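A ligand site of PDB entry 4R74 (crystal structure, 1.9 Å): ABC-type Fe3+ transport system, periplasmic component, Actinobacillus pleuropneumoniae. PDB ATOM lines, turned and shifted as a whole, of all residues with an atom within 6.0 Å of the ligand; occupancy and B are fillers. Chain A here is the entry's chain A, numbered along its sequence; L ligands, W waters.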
ATOM      1  N   SER A  11     -12.204   0.975  -2.522  1.00  0.00           N
ATOM      2  CA  SER A  11     -11.654  -0.278  -2.020  1.00  0.00           C
ATOM      3  C   SER A  11     -11.880  -0.468  -0.526  1.00  0.00           C
ATOM      4  O   SER A  11     -11.294  -1.364   0.084  1.00  0.00           O
ATOM      5  CB  SER A  11     -10.155  -0.373  -2.341  1.00  0.00           C
ATOM      6  OG  SER A  11      -9.925  -0.379  -3.740  1.00  0.00           O
ATOM      7  N   ALA A  12     -12.725   0.362   0.080  1.00  0.00           N
ATOM      8  CA  ALA A  12     -13.149   0.141   1.462  1.00  0.00           C
ATOM      9  C   ALA A  12     -14.389  -0.756   1.445  1.00  0.00           C
ATOM     10  O   ALA A  12     -14.713  -1.336   0.422  1.00  0.00           O
ATOM     11  CB  ALA A  12     -13.416   1.463   2.181  1.00  0.00           C
ATOM     12  N   THR A  13     -15.088  -0.870   2.567  1.00  0.00           N
ATOM     13  CA  THR A  13     -16.315  -1.670   2.571  1.00  0.00           C
ATOM     14  C   THR A  13     -17.441  -0.942   1.837  1.00  0.00           C
ATOM     15  O   THR A  13     -17.451   0.285   1.753  1.00  0.00           O
ATOM     16  CB  THR A  13     -16.797  -1.993   3.987  1.00  0.00           C
ATOM     17  OG1 THR A  13     -16.981  -0.791   4.728  1.00  0.00           O
ATOM     18  CG2 THR A  13     -15.773  -2.872   4.702  1.00  0.00           C
ATOM     19  N   ARG A  36     -17.046  -0.979  -6.199  1.00  0.00           N
ATOM     20  CA  ARG A  36     -16.224  -1.455  -5.099  1.00  0.00           C
ATOM     21  C   ARG A  36     -15.422  -2.698  -5.486  1.00  0.00           C
ATOM     22  O   ARG A  36     -15.966  -3.672  -5.995  1.00  0.00           O
ATOM     23  CB  ARG A  36     -17.095  -1.754  -3.881  1.00  0.00           C
ATOM     24  CG  ARG A  36     -16.338  -1.859  -2.587  1.00  0.00           C
ATOM     25  CD  ARG A  36     -16.698  -3.144  -1.860  1.00  0.00           C
ATOM     26  NE  ARG A  36     -15.941  -4.274  -2.377  1.00  0.00           N
ATOM     27  CZ  ARG A  36     -14.677  -4.525  -2.064  1.00  0.00           C
ATOM     28  NH1 ARG A  36     -14.063  -5.585  -2.583  1.00  0.00           N
ATOM     29  NH2 ARG A  36     -14.013  -3.727  -1.232  1.00  0.00           N
ATOM     30  N   ASN A  37     -14.114  -2.659  -5.237  1.00  0.00           N
ATOM     31  CA  ASN A  37     -13.291  -3.838  -5.451  1.00  0.00           C
ATOM     32  C   ASN A  37     -12.063  -3.763  -4.564  1.00  0.00           C
ATOM     33  O   ASN A  37     -11.747  -2.695  -4.044  1.00  0.00           O
ATOM     34  CB  ASN A  37     -12.912  -3.986  -6.922  1.00  0.00           C
ATOM     35  CG  ASN A  37     -13.133  -5.405  -7.438  1.00  0.00           C
ATOM     36  OD1 ASN A  37     -12.860  -6.376  -6.728  1.00  0.00           O
ATOM     37  ND2 ASN A  37     -13.631  -5.521  -8.660  1.00  0.00           N
ATOM     38  N   GLY A  38     -11.404  -4.907  -4.379  1.00  0.00           N
ATOM     39  CA  GLY A  38     -10.197  -4.954  -3.553  1.00  0.00           C
ATOM     40  C   GLY A  38      -9.097  -4.027  -4.037  1.00  0.00           C
ATOM     41  O   GLY A  38      -9.090  -3.596  -5.205  1.00  0.00           O
ATOM     42  N   SER A  39      -8.184  -3.701  -3.135  1.00  0.00           N
ATOM     43  CA  SER A  39      -7.062  -2.801  -3.436  1.00  0.00           C
ATOM     44  C   SER A  39      -6.209  -3.331  -4.586  1.00  0.00           C
ATOM     45  O   SER A  39      -5.846  -2.576  -5.495  1.00  0.00           O
ATOM     46  CB  SER A  39      -6.182  -2.591  -2.208  1.00  0.00           C
ATOM     47  OG  SER A  39      -6.954  -2.311  -1.048  1.00  0.00           O
ATOM     48  N   GLY A  40      -5.854  -4.607  -4.531  1.00  0.00           N
ATOM     49  CA  GLY A  40      -5.102  -5.230  -5.619  1.00  0.00           C
ATOM     50  C   GLY A  40      -5.920  -5.378  -6.893  1.00  0.00           C
ATOM     51  O   GLY A  40      -5.435  -5.079  -7.997  1.00  0.00           O
ATOM     52  N   GLY A  60      -9.989   4.661  -0.666  1.00  0.00           N
ATOM     53  CA  GLY A  60      -9.923   3.576   0.298  1.00  0.00           C
ATOM     54  C   GLY A  60      -9.063   2.410  -0.155  1.00  0.00           C
ATOM     55  O   GLY A  60      -8.442   2.450  -1.219  1.00  0.00           O
ATOM     56  N   GLY A  61      -9.055   1.335   0.630  1.00  0.00           N
ATOM     57  CA  GLY A  61      -8.133   0.237   0.367  1.00  0.00           C
ATOM     58  C   GLY A  61      -6.766   0.688   0.826  1.00  0.00           C
ATOM     59  O   GLY A  61      -6.586   1.816   1.278  1.00  0.00           O
ATOM     60  N   THR A  62      -5.783  -0.200   0.703  1.00  0.00           N
ATOM     61  CA  THR A  62      -4.476   0.065   1.276  1.00  0.00           C
ATOM     62  C   THR A  62      -3.641   0.978   0.387  1.00  0.00           C
ATOM     63  O   THR A  62      -3.864   1.057  -0.833  1.00  0.00           O
ATOM     64  CB  THR A  62      -3.702  -1.233   1.502  1.00  0.00           C
ATOM     65  OG1 THR A  62      -3.482  -1.844   0.223  1.00  0.00           O
ATOM     66  CG2 THR A  62      -4.489  -2.164   2.426  1.00  0.00           C
ATOM     67  N   TYR A 105      -6.873   7.273   6.275  1.00  0.00           N
ATOM     68  CA  TYR A 105      -7.072   6.570   7.526  1.00  0.00           C
ATOM     69  C   TYR A 105      -5.935   5.621   7.828  1.00  0.00           C
ATOM     70  O   TYR A 105      -5.031   5.435   7.008  1.00  0.00           O
ATOM     71  CB  TYR A 105      -8.424   5.825   7.562  1.00  0.00           C
ATOM     72  CG  TYR A 105      -8.687   4.782   6.483  1.00  0.00           C
ATOM     73  CD1 TYR A 105      -8.006   3.567   6.452  1.00  0.00           C
ATOM     74  CD2 TYR A 105      -9.694   4.996   5.531  1.00  0.00           C
ATOM     75  CE1 TYR A 105      -8.302   2.595   5.460  1.00  0.00           C
ATOM     76  CE2 TYR A 105      -9.989   4.042   4.556  1.00  0.00           C
ATOM     77  CZ  TYR A 105      -9.286   2.846   4.521  1.00  0.00           C
ATOM     78  OH  TYR A 105      -9.586   1.913   3.542  1.00  0.00           O
ATOM     79  N   GLY A 107      -5.161   1.632   9.582  1.00  0.00           N
ATOM     80  CA  GLY A 107      -5.751   0.389  10.049  1.00  0.00           C
ATOM     81  C   GLY A 107      -4.683  -0.521  10.604  1.00  0.00           C
ATOM     82  O   GLY A 107      -3.642  -0.703   9.976  1.00  0.00           O
ATOM     83  N   ALA A 145      -6.627 -13.136   3.677  1.00  0.00           N
ATOM     84  CA  ALA A 145      -6.909 -12.865   2.275  1.00  0.00           C
ATOM     85  C   ALA A 145      -5.738 -13.235   1.346  1.00  0.00           C
ATOM     86  O   ALA A 145      -4.641 -13.575   1.797  1.00  0.00           O
ATOM     87  CB  ALA A 145      -7.303 -11.395   2.088  1.00  0.00           C
ATOM     88  N   SER A 149      -5.643 -10.180  -4.880  1.00  0.00           N
ATOM     89  CA  SER A 149      -6.797  -9.261  -4.895  1.00  0.00           C
ATOM     90  C   SER A 149      -6.753  -8.265  -3.745  1.00  0.00           C
ATOM     91  O   SER A 149      -7.207  -7.123  -3.873  1.00  0.00           O
ATOM     92  CB  SER A 149      -8.109 -10.041  -4.848  1.00  0.00           C
ATOM     93  OG  SER A 149      -8.102 -11.021  -3.807  1.00  0.00           O
ATOM     94  N   SER A 150      -6.213  -8.707  -2.607  1.00  0.00           N
ATOM     95  CA  SER A 150      -6.375  -7.986  -1.347  1.00  0.00           C
ATOM     96  C   SER A 150      -5.153  -7.178  -0.915  1.00  0.00           C
ATOM     97  O   SER A 150      -4.047  -7.727  -0.778  1.00  0.00           O
ATOM     98  CB  SER A 150      -6.725  -8.973  -0.235  1.00  0.00           C
ATOM     99  OG  SER A 150      -6.517  -8.424   1.058  1.00  0.00           O
ATOM    100  N   GLY A 151      -5.354  -5.896  -0.656  1.00  0.00           N
ATOM    101  CA  GLY A 151      -4.305  -5.078  -0.071  1.00  0.00           C
ATOM    102  C   GLY A 151      -3.930  -5.527   1.330  1.00  0.00           C
ATOM    103  O   GLY A 151      -2.759  -5.460   1.728  1.00  0.00           O
ATOM    104  N   THR A 152      -4.920  -5.977   2.101  1.00  0.00           N
ATOM    105  CA  THR A 152      -4.682  -6.480   3.454  1.00  0.00           C
ATOM    106  C   THR A 152      -3.647  -7.593   3.458  1.00  0.00           C
ATOM    107  O   THR A 152      -2.715  -7.620   4.269  1.00  0.00           O
ATOM    108  CB  THR A 152      -5.966  -7.033   4.091  1.00  0.00           C
ATOM    109  OG1 THR A 152      -6.993  -6.036   4.042  1.00  0.00           O
ATOM    110  CG2 THR A 152      -5.688  -7.432   5.539  1.00  0.00           C
ATOM    111  N   ALA A 153      -3.814  -8.522   2.534  1.00  0.00           N
ATOM    112  CA  ALA A 153      -2.921  -9.662   2.444  1.00  0.00           C
ATOM    113  C   ALA A 153      -1.502  -9.184   2.122  1.00  0.00           C
ATOM    114  O   ALA A 153      -0.536  -9.748   2.637  1.00  0.00           O
ATOM    115  CB  ALA A 153      -3.414 -10.634   1.402  1.00  0.00           C
ATOM    116  N   LYS A 185     -10.810 -13.739  -1.107  1.00  0.00           N
ATOM    117  CA  LYS A 185     -10.629 -12.669  -2.085  1.00  0.00           C
ATOM    118  C   LYS A 185     -10.531 -11.307  -1.396  1.00  0.00           C
ATOM    119  O   LYS A 185      -9.670 -10.497  -1.721  1.00  0.00           O
ATOM    120  CB  LYS A 185     -11.777 -12.669  -3.101  1.00  0.00           C
ATOM    121  CG  LYS A 185     -11.623 -11.615  -4.168  1.00  0.00           C
ATOM    122  CD  LYS A 185     -12.632 -11.793  -5.283  1.00  0.00           C
ATOM    123  CE  LYS A 185     -12.614 -10.622  -6.253  1.00  0.00           C
ATOM    124  NZ  LYS A 185     -13.084  -9.381  -5.582  1.00  0.00           N
ATOM    125  N   SER A 186     -11.421 -11.073  -0.425  1.00  0.00           N
ATOM    126  CA  SER A 186     -11.478  -9.792   0.268  1.00  0.00           C
ATOM    127  C   SER A 186     -10.758  -9.800   1.616  1.00  0.00           C
ATOM    128  O   SER A 186     -10.792 -10.794   2.347  1.00  0.00           O
ATOM    129  CB  SER A 186     -12.928  -9.360   0.473  1.00  0.00           C
ATOM    130  OG  SER A 186     -13.607  -9.330  -0.757  1.00  0.00           O
ATOM    131  N   GLY A 187     -10.120  -8.675   1.942  1.00  0.00           N
ATOM    132  CA  GLY A 187      -9.353  -8.561   3.188  1.00  0.00           C
ATOM    133  C   GLY A 187     -10.230  -8.740   4.423  1.00  0.00           C
ATOM    134  O   GLY A 187      -9.771  -9.243   5.456  1.00  0.00           O
ATOM    135  N   ILE A 188     -11.496  -8.336   4.310  1.00  0.00           N
ATOM    136  CA  ILE A 188     -12.413  -8.306   5.444  1.00  0.00           C
ATOM    137  C   ILE A 188     -13.117  -9.647   5.663  1.00  0.00           C
ATOM    138  O   ILE A 188     -13.731  -9.880   6.722  1.00  0.00           O
ATOM    139  CB  ILE A 188     -13.479  -7.214   5.243  1.00  0.00           C
ATOM    140  CG1 ILE A 188     -14.174  -6.891   6.562  1.00  0.00           C
ATOM    141  CG2 ILE A 188     -14.493  -7.649   4.163  1.00  0.00           C
ATOM    142  CD1 ILE A 188     -15.194  -5.815   6.453  1.00  0.00           C
ATOM    143  N   PHE A 205      -7.332  -6.304   9.308  1.00  0.00           N
ATOM    144  CA  PHE A 205      -7.233  -5.034  10.006  1.00  0.00           C
ATOM    145  C   PHE A 205      -8.229  -5.021  11.156  1.00  0.00           C
ATOM    146  O   PHE A 205      -9.399  -5.375  10.989  1.00  0.00           O
ATOM    147  CB  PHE A 205      -7.443  -3.869   9.040  1.00  0.00           C
ATOM    148  CG  PHE A 205      -6.357  -3.781   7.994  1.00  0.00           C
ATOM    149  CD1 PHE A 205      -5.016  -3.824   8.375  1.00  0.00           C
ATOM    150  CD2 PHE A 205      -6.669  -3.718   6.647  1.00  0.00           C
ATOM    151  CE1 PHE A 205      -4.006  -3.762   7.408  1.00  0.00           C
ATOM    152  CE2 PHE A 205      -5.666  -3.658   5.687  1.00  0.00           C
ATOM    153  CZ  PHE A 205      -4.339  -3.690   6.069  1.00  0.00           C
ATOM    154  N   HIS A 207      -9.857  -2.908  13.056  1.00  0.00           N
ATOM    155  CA  HIS A 207     -11.107  -2.126  13.062  1.00  0.00           C
ATOM    156  C   HIS A 207     -12.292  -2.889  12.437  1.00  0.00           C
ATOM    157  O   HIS A 207     -13.459  -2.685  12.828  1.00  0.00           O
ATOM    158  CB  HIS A 207     -10.899  -0.783  12.351  1.00  0.00           C
ATOM    159  CG  HIS A 207     -10.450  -0.912  10.928  1.00  0.00           C
ATOM    160  ND1 HIS A 207      -9.143  -0.741  10.538  1.00  0.00           N
ATOM    161  CD2 HIS A 207     -11.152  -1.169   9.800  1.00  0.00           C
ATOM    162  CE1 HIS A 207      -9.047  -0.914   9.231  1.00  0.00           C
ATOM    163  NE2 HIS A 207     -10.257  -1.169   8.749  1.00  0.00           N
ATOM    164  N   ASP A 208     -12.028  -3.760  11.467  1.00  0.00           N
ATOM    165  CA  ASP A 208     -13.100  -4.601  10.914  1.00  0.00           C
ATOM    166  C   ASP A 208     -13.610  -5.562  11.988  1.00  0.00           C
ATOM    167  O   ASP A 208     -14.820  -5.756  12.143  1.00  0.00           O
ATOM    168  CB  ASP A 208     -12.630  -5.365   9.673  1.00  0.00           C
ATOM    169  CG  ASP A 208     -12.311  -4.438   8.495  1.00  0.00           C
ATOM    170  OD1 ASP A 208     -13.022  -3.427   8.345  1.00  0.00           O
ATOM    171  OD2 ASP A 208     -11.352  -4.718   7.741  1.00  0.00           O
ATOM    172  N   GLU A 231      -1.943  -0.440   7.705  1.00  0.00           N
ATOM    173  CA  GLU A 231      -2.215   0.207   6.428  1.00  0.00           C
ATOM    174  C   GLU A 231      -2.386   1.694   6.660  1.00  0.00           C
ATOM    175  O   GLU A 231      -2.805   2.114   7.740  1.00  0.00           O
ATOM    176  CB  GLU A 231      -3.483  -0.341   5.759  1.00  0.00           C
ATOM    177  CG  GLU A 231      -4.740  -0.205   6.666  1.00  0.00           C
ATOM    178  CD  GLU A 231      -6.082  -0.322   5.920  1.00  0.00           C
ATOM    179  OE1 GLU A 231      -6.103  -0.222   4.668  1.00  0.00           O
ATOM    180  OE2 GLU A 231      -7.120  -0.484   6.614  1.00  0.00           O
ATOM    181  N   GLY A 233      -4.973   4.082   4.561  1.00  0.00           N
ATOM    182  CA  GLY A 233      -5.984   4.097   3.517  1.00  0.00           C
ATOM    183  C   GLY A 233      -5.617   5.185   2.534  1.00  0.00           C
ATOM    184  O   GLY A 233      -5.136   6.239   2.937  1.00  0.00           O
ATOM    185  N   ALA A 269     -17.342   2.430   9.749  1.00  0.00           N
ATOM    186  CA  ALA A 269     -15.958   2.128   9.452  1.00  0.00           C
ATOM    187  C   ALA A 269     -15.080   2.744  10.530  1.00  0.00           C
ATOM    188  O   ALA A 269     -15.062   3.965  10.696  1.00  0.00           O
ATOM    189  CB  ALA A 269     -15.590   2.665   8.077  1.00  0.00           C
ATOM    190  N   GLN A 271     -11.712   2.821  11.249  1.00  0.00           N
ATOM    191  CA  GLN A 271     -10.290   3.121  11.110  1.00  0.00           C
ATOM    192  C   GLN A 271      -9.913   4.367  11.915  1.00  0.00           C
ATOM    193  O   GLN A 271     -10.756   5.207  12.244  1.00  0.00           O
ATOM    194  CB  GLN A 271      -9.900   3.336   9.648  1.00  0.00           C
ATOM    195  CG  GLN A 271     -10.206   2.159   8.748  1.00  0.00           C
ATOM    196  CD  GLN A 271     -11.536   2.318   8.048  1.00  0.00           C
ATOM    197  OE1 GLN A 271     -12.403   3.081   8.494  1.00  0.00           O
ATOM    198  NE2 GLN A 271     -11.711   1.617   6.942  1.00  0.00           N
HETATM  199  O1  LIG L   1     -12.368  -1.691   6.600  1.00  0.00           O
HETATM  200  C1  LIG L   1     -12.107  -2.382   5.434  1.00  0.00           C
HETATM  201  C2  LIG L   1     -10.660  -2.511   5.099  1.00  0.00           C
HETATM  202  O2  LIG L   1     -10.021  -3.191   6.150  1.00  0.00           O
HETATM  203  C3  LIG L   1     -10.064  -1.193   4.879  1.00  0.00           C
HETATM  204  O3  LIG L   1      -9.699  -0.489   6.014  1.00  0.00           O
HETATM  205  C4  LIG L   1      -8.905  -1.579   4.069  1.00  0.00           C
HETATM  206  O4  LIG L   1      -8.397  -0.453   3.461  1.00  0.00           O
HETATM  207  C5  LIG L   1      -9.564  -2.476   3.074  1.00  0.00           C
HETATM  208  O5  LIG L   1     -10.469  -3.232   3.826  1.00  0.00           O
HETATM  209  C6  LIG L   1      -8.685  -3.392   2.278  1.00  0.00           C
HETATM  210  O6  LIG L   1      -9.407  -4.284   1.496  1.00  0.00           O
HETATM  211  P1  LIG L   1      -8.732  -5.405   0.670  1.00  0.00           P
HETATM  212  O7  LIG L   1      -7.973  -4.756  -0.467  1.00  0.00           O
HETATM  213  O8  LIG L   1      -7.800  -6.234   1.497  1.00  0.00           O
HETATM  214  O9  LIG L   1      -9.862  -6.265   0.127  1.00  0.00           O
HETATM  215  O   HOH W   1     -14.226   0.268   5.519  1.00  0.00           O
HETATM  216  O   HOH W   2      -9.778  -7.793  -2.172  1.00  0.00           O
HETATM  217  O   HOH W   3      -9.403  -5.936   5.236  1.00  0.00           O
HETATM  218  O   HOH W   4     -11.863  -5.839   2.461  1.00  0.00           O
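Water W2 lies within hydrogen-bond range of O of Lys 185 (2.7 Å), O9 of the ligand (2.8 Å) and O of Ser 149 (3.2 Å). Water W1 lies within hydrogen-bond range of O1 of the ligand, OG1 of Thr 13 and NE2 of Gln 271. Water W3 lies within hydrogen-bond range of the side-chain hydroxyl of Thr 152, an oxygen (O2) of the ligand, the backbone NH of Ile 188, the backbone carbonyl oxygen of Gly 187 and the side-chain carboxylate of Asp 208. Water W4 lies within hydrogen-bond range of O6 of the ligand, N of Ile 188 and N of Gly 187.
Merely in contact with the ligand: Phe 205, Ser 11, Thr 13, Thr 62, Gly 38 and Ser 186. Of the 30 residues printed, 17 come within 4 Å of the ligand.
O3 of the ligand sits at hydrogen-bond distance from NE2 of His 207 (2.9 Å). The side-chain amide nitrogen of Gln 271 lies within hydrogen-bond range of an oxygen (O3) of the ligand. O4 of the ligand sits at hydrogen-bond distance from OH of Tyr 105 (2.6 Å). OD1 of Asp 208 sits at hydrogen-bond distance from O1 of the ligand, at 2.5 Å. The backbone NH (N) of Thr 152 lies within hydrogen-bond range of an oxygen (O8) of the ligand, 3.0 Å away. The backbone NH (N) of Gly 61 lies close to an oxygen (O4) of the ligand, at 3.4 Å. The backbone NH (N) of Ser 39 lies within hydrogen-bond range of an oxygen (O7) of the ligand. O8 of the ligand lies within hydrogen-bond range of OG1 of Thr 152, 2.7 Å away. An oxygen (O7) of the ligand is in hydrogen-bond range of the backbone NH of Gly 151 (2.9 Å). The side-chain hydroxyl (OG) of Ser 39 lies within hydrogen-bond range of an oxygen (O7) of the ligand, at 2.7 Å. N of Gly 187 sits at hydrogen-bond distance from O9 of the ligand (3.0 Å). O8 of the ligand sits at hydrogen-bond distance from OG of Ser 150, at 2.6 Å. The side-chain carboxylate (OE1) of Glu 231 is in hydrogen-bond range of an oxygen (O4) of the ligand, 2.6 Å away.
The side-chain hydroxyl (OG) of Ser 150 lies within hydrogen-bond range of the backbone NH (N) of Thr 152 (3.1 Å). OG of Ser 11 is in hydrogen-bond range of O of Asn 37. N of Glu 231 lies within hydrogen-bond range of O of Gly 107 (2.8 Å). The backbone NH (N) of Thr 62 lies within hydrogen-bond range of the side-chain hydroxyl (OG) of Ser 39, 3.0 Å away. The backbone carbonyl oxygen of Tyr 105 lies within hydrogen-bond range of the backbone NH of Gly 233 (2.8 Å). The side-chain hydroxyl of Ser 150 is in hydrogen-bond range of the backbone NH of Ala 153. The backbone NH (N) of Gly 61 lies within hydrogen-bond range of the side-chain hydroxyl (OH) of Tyr 105 (3.0 Å).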
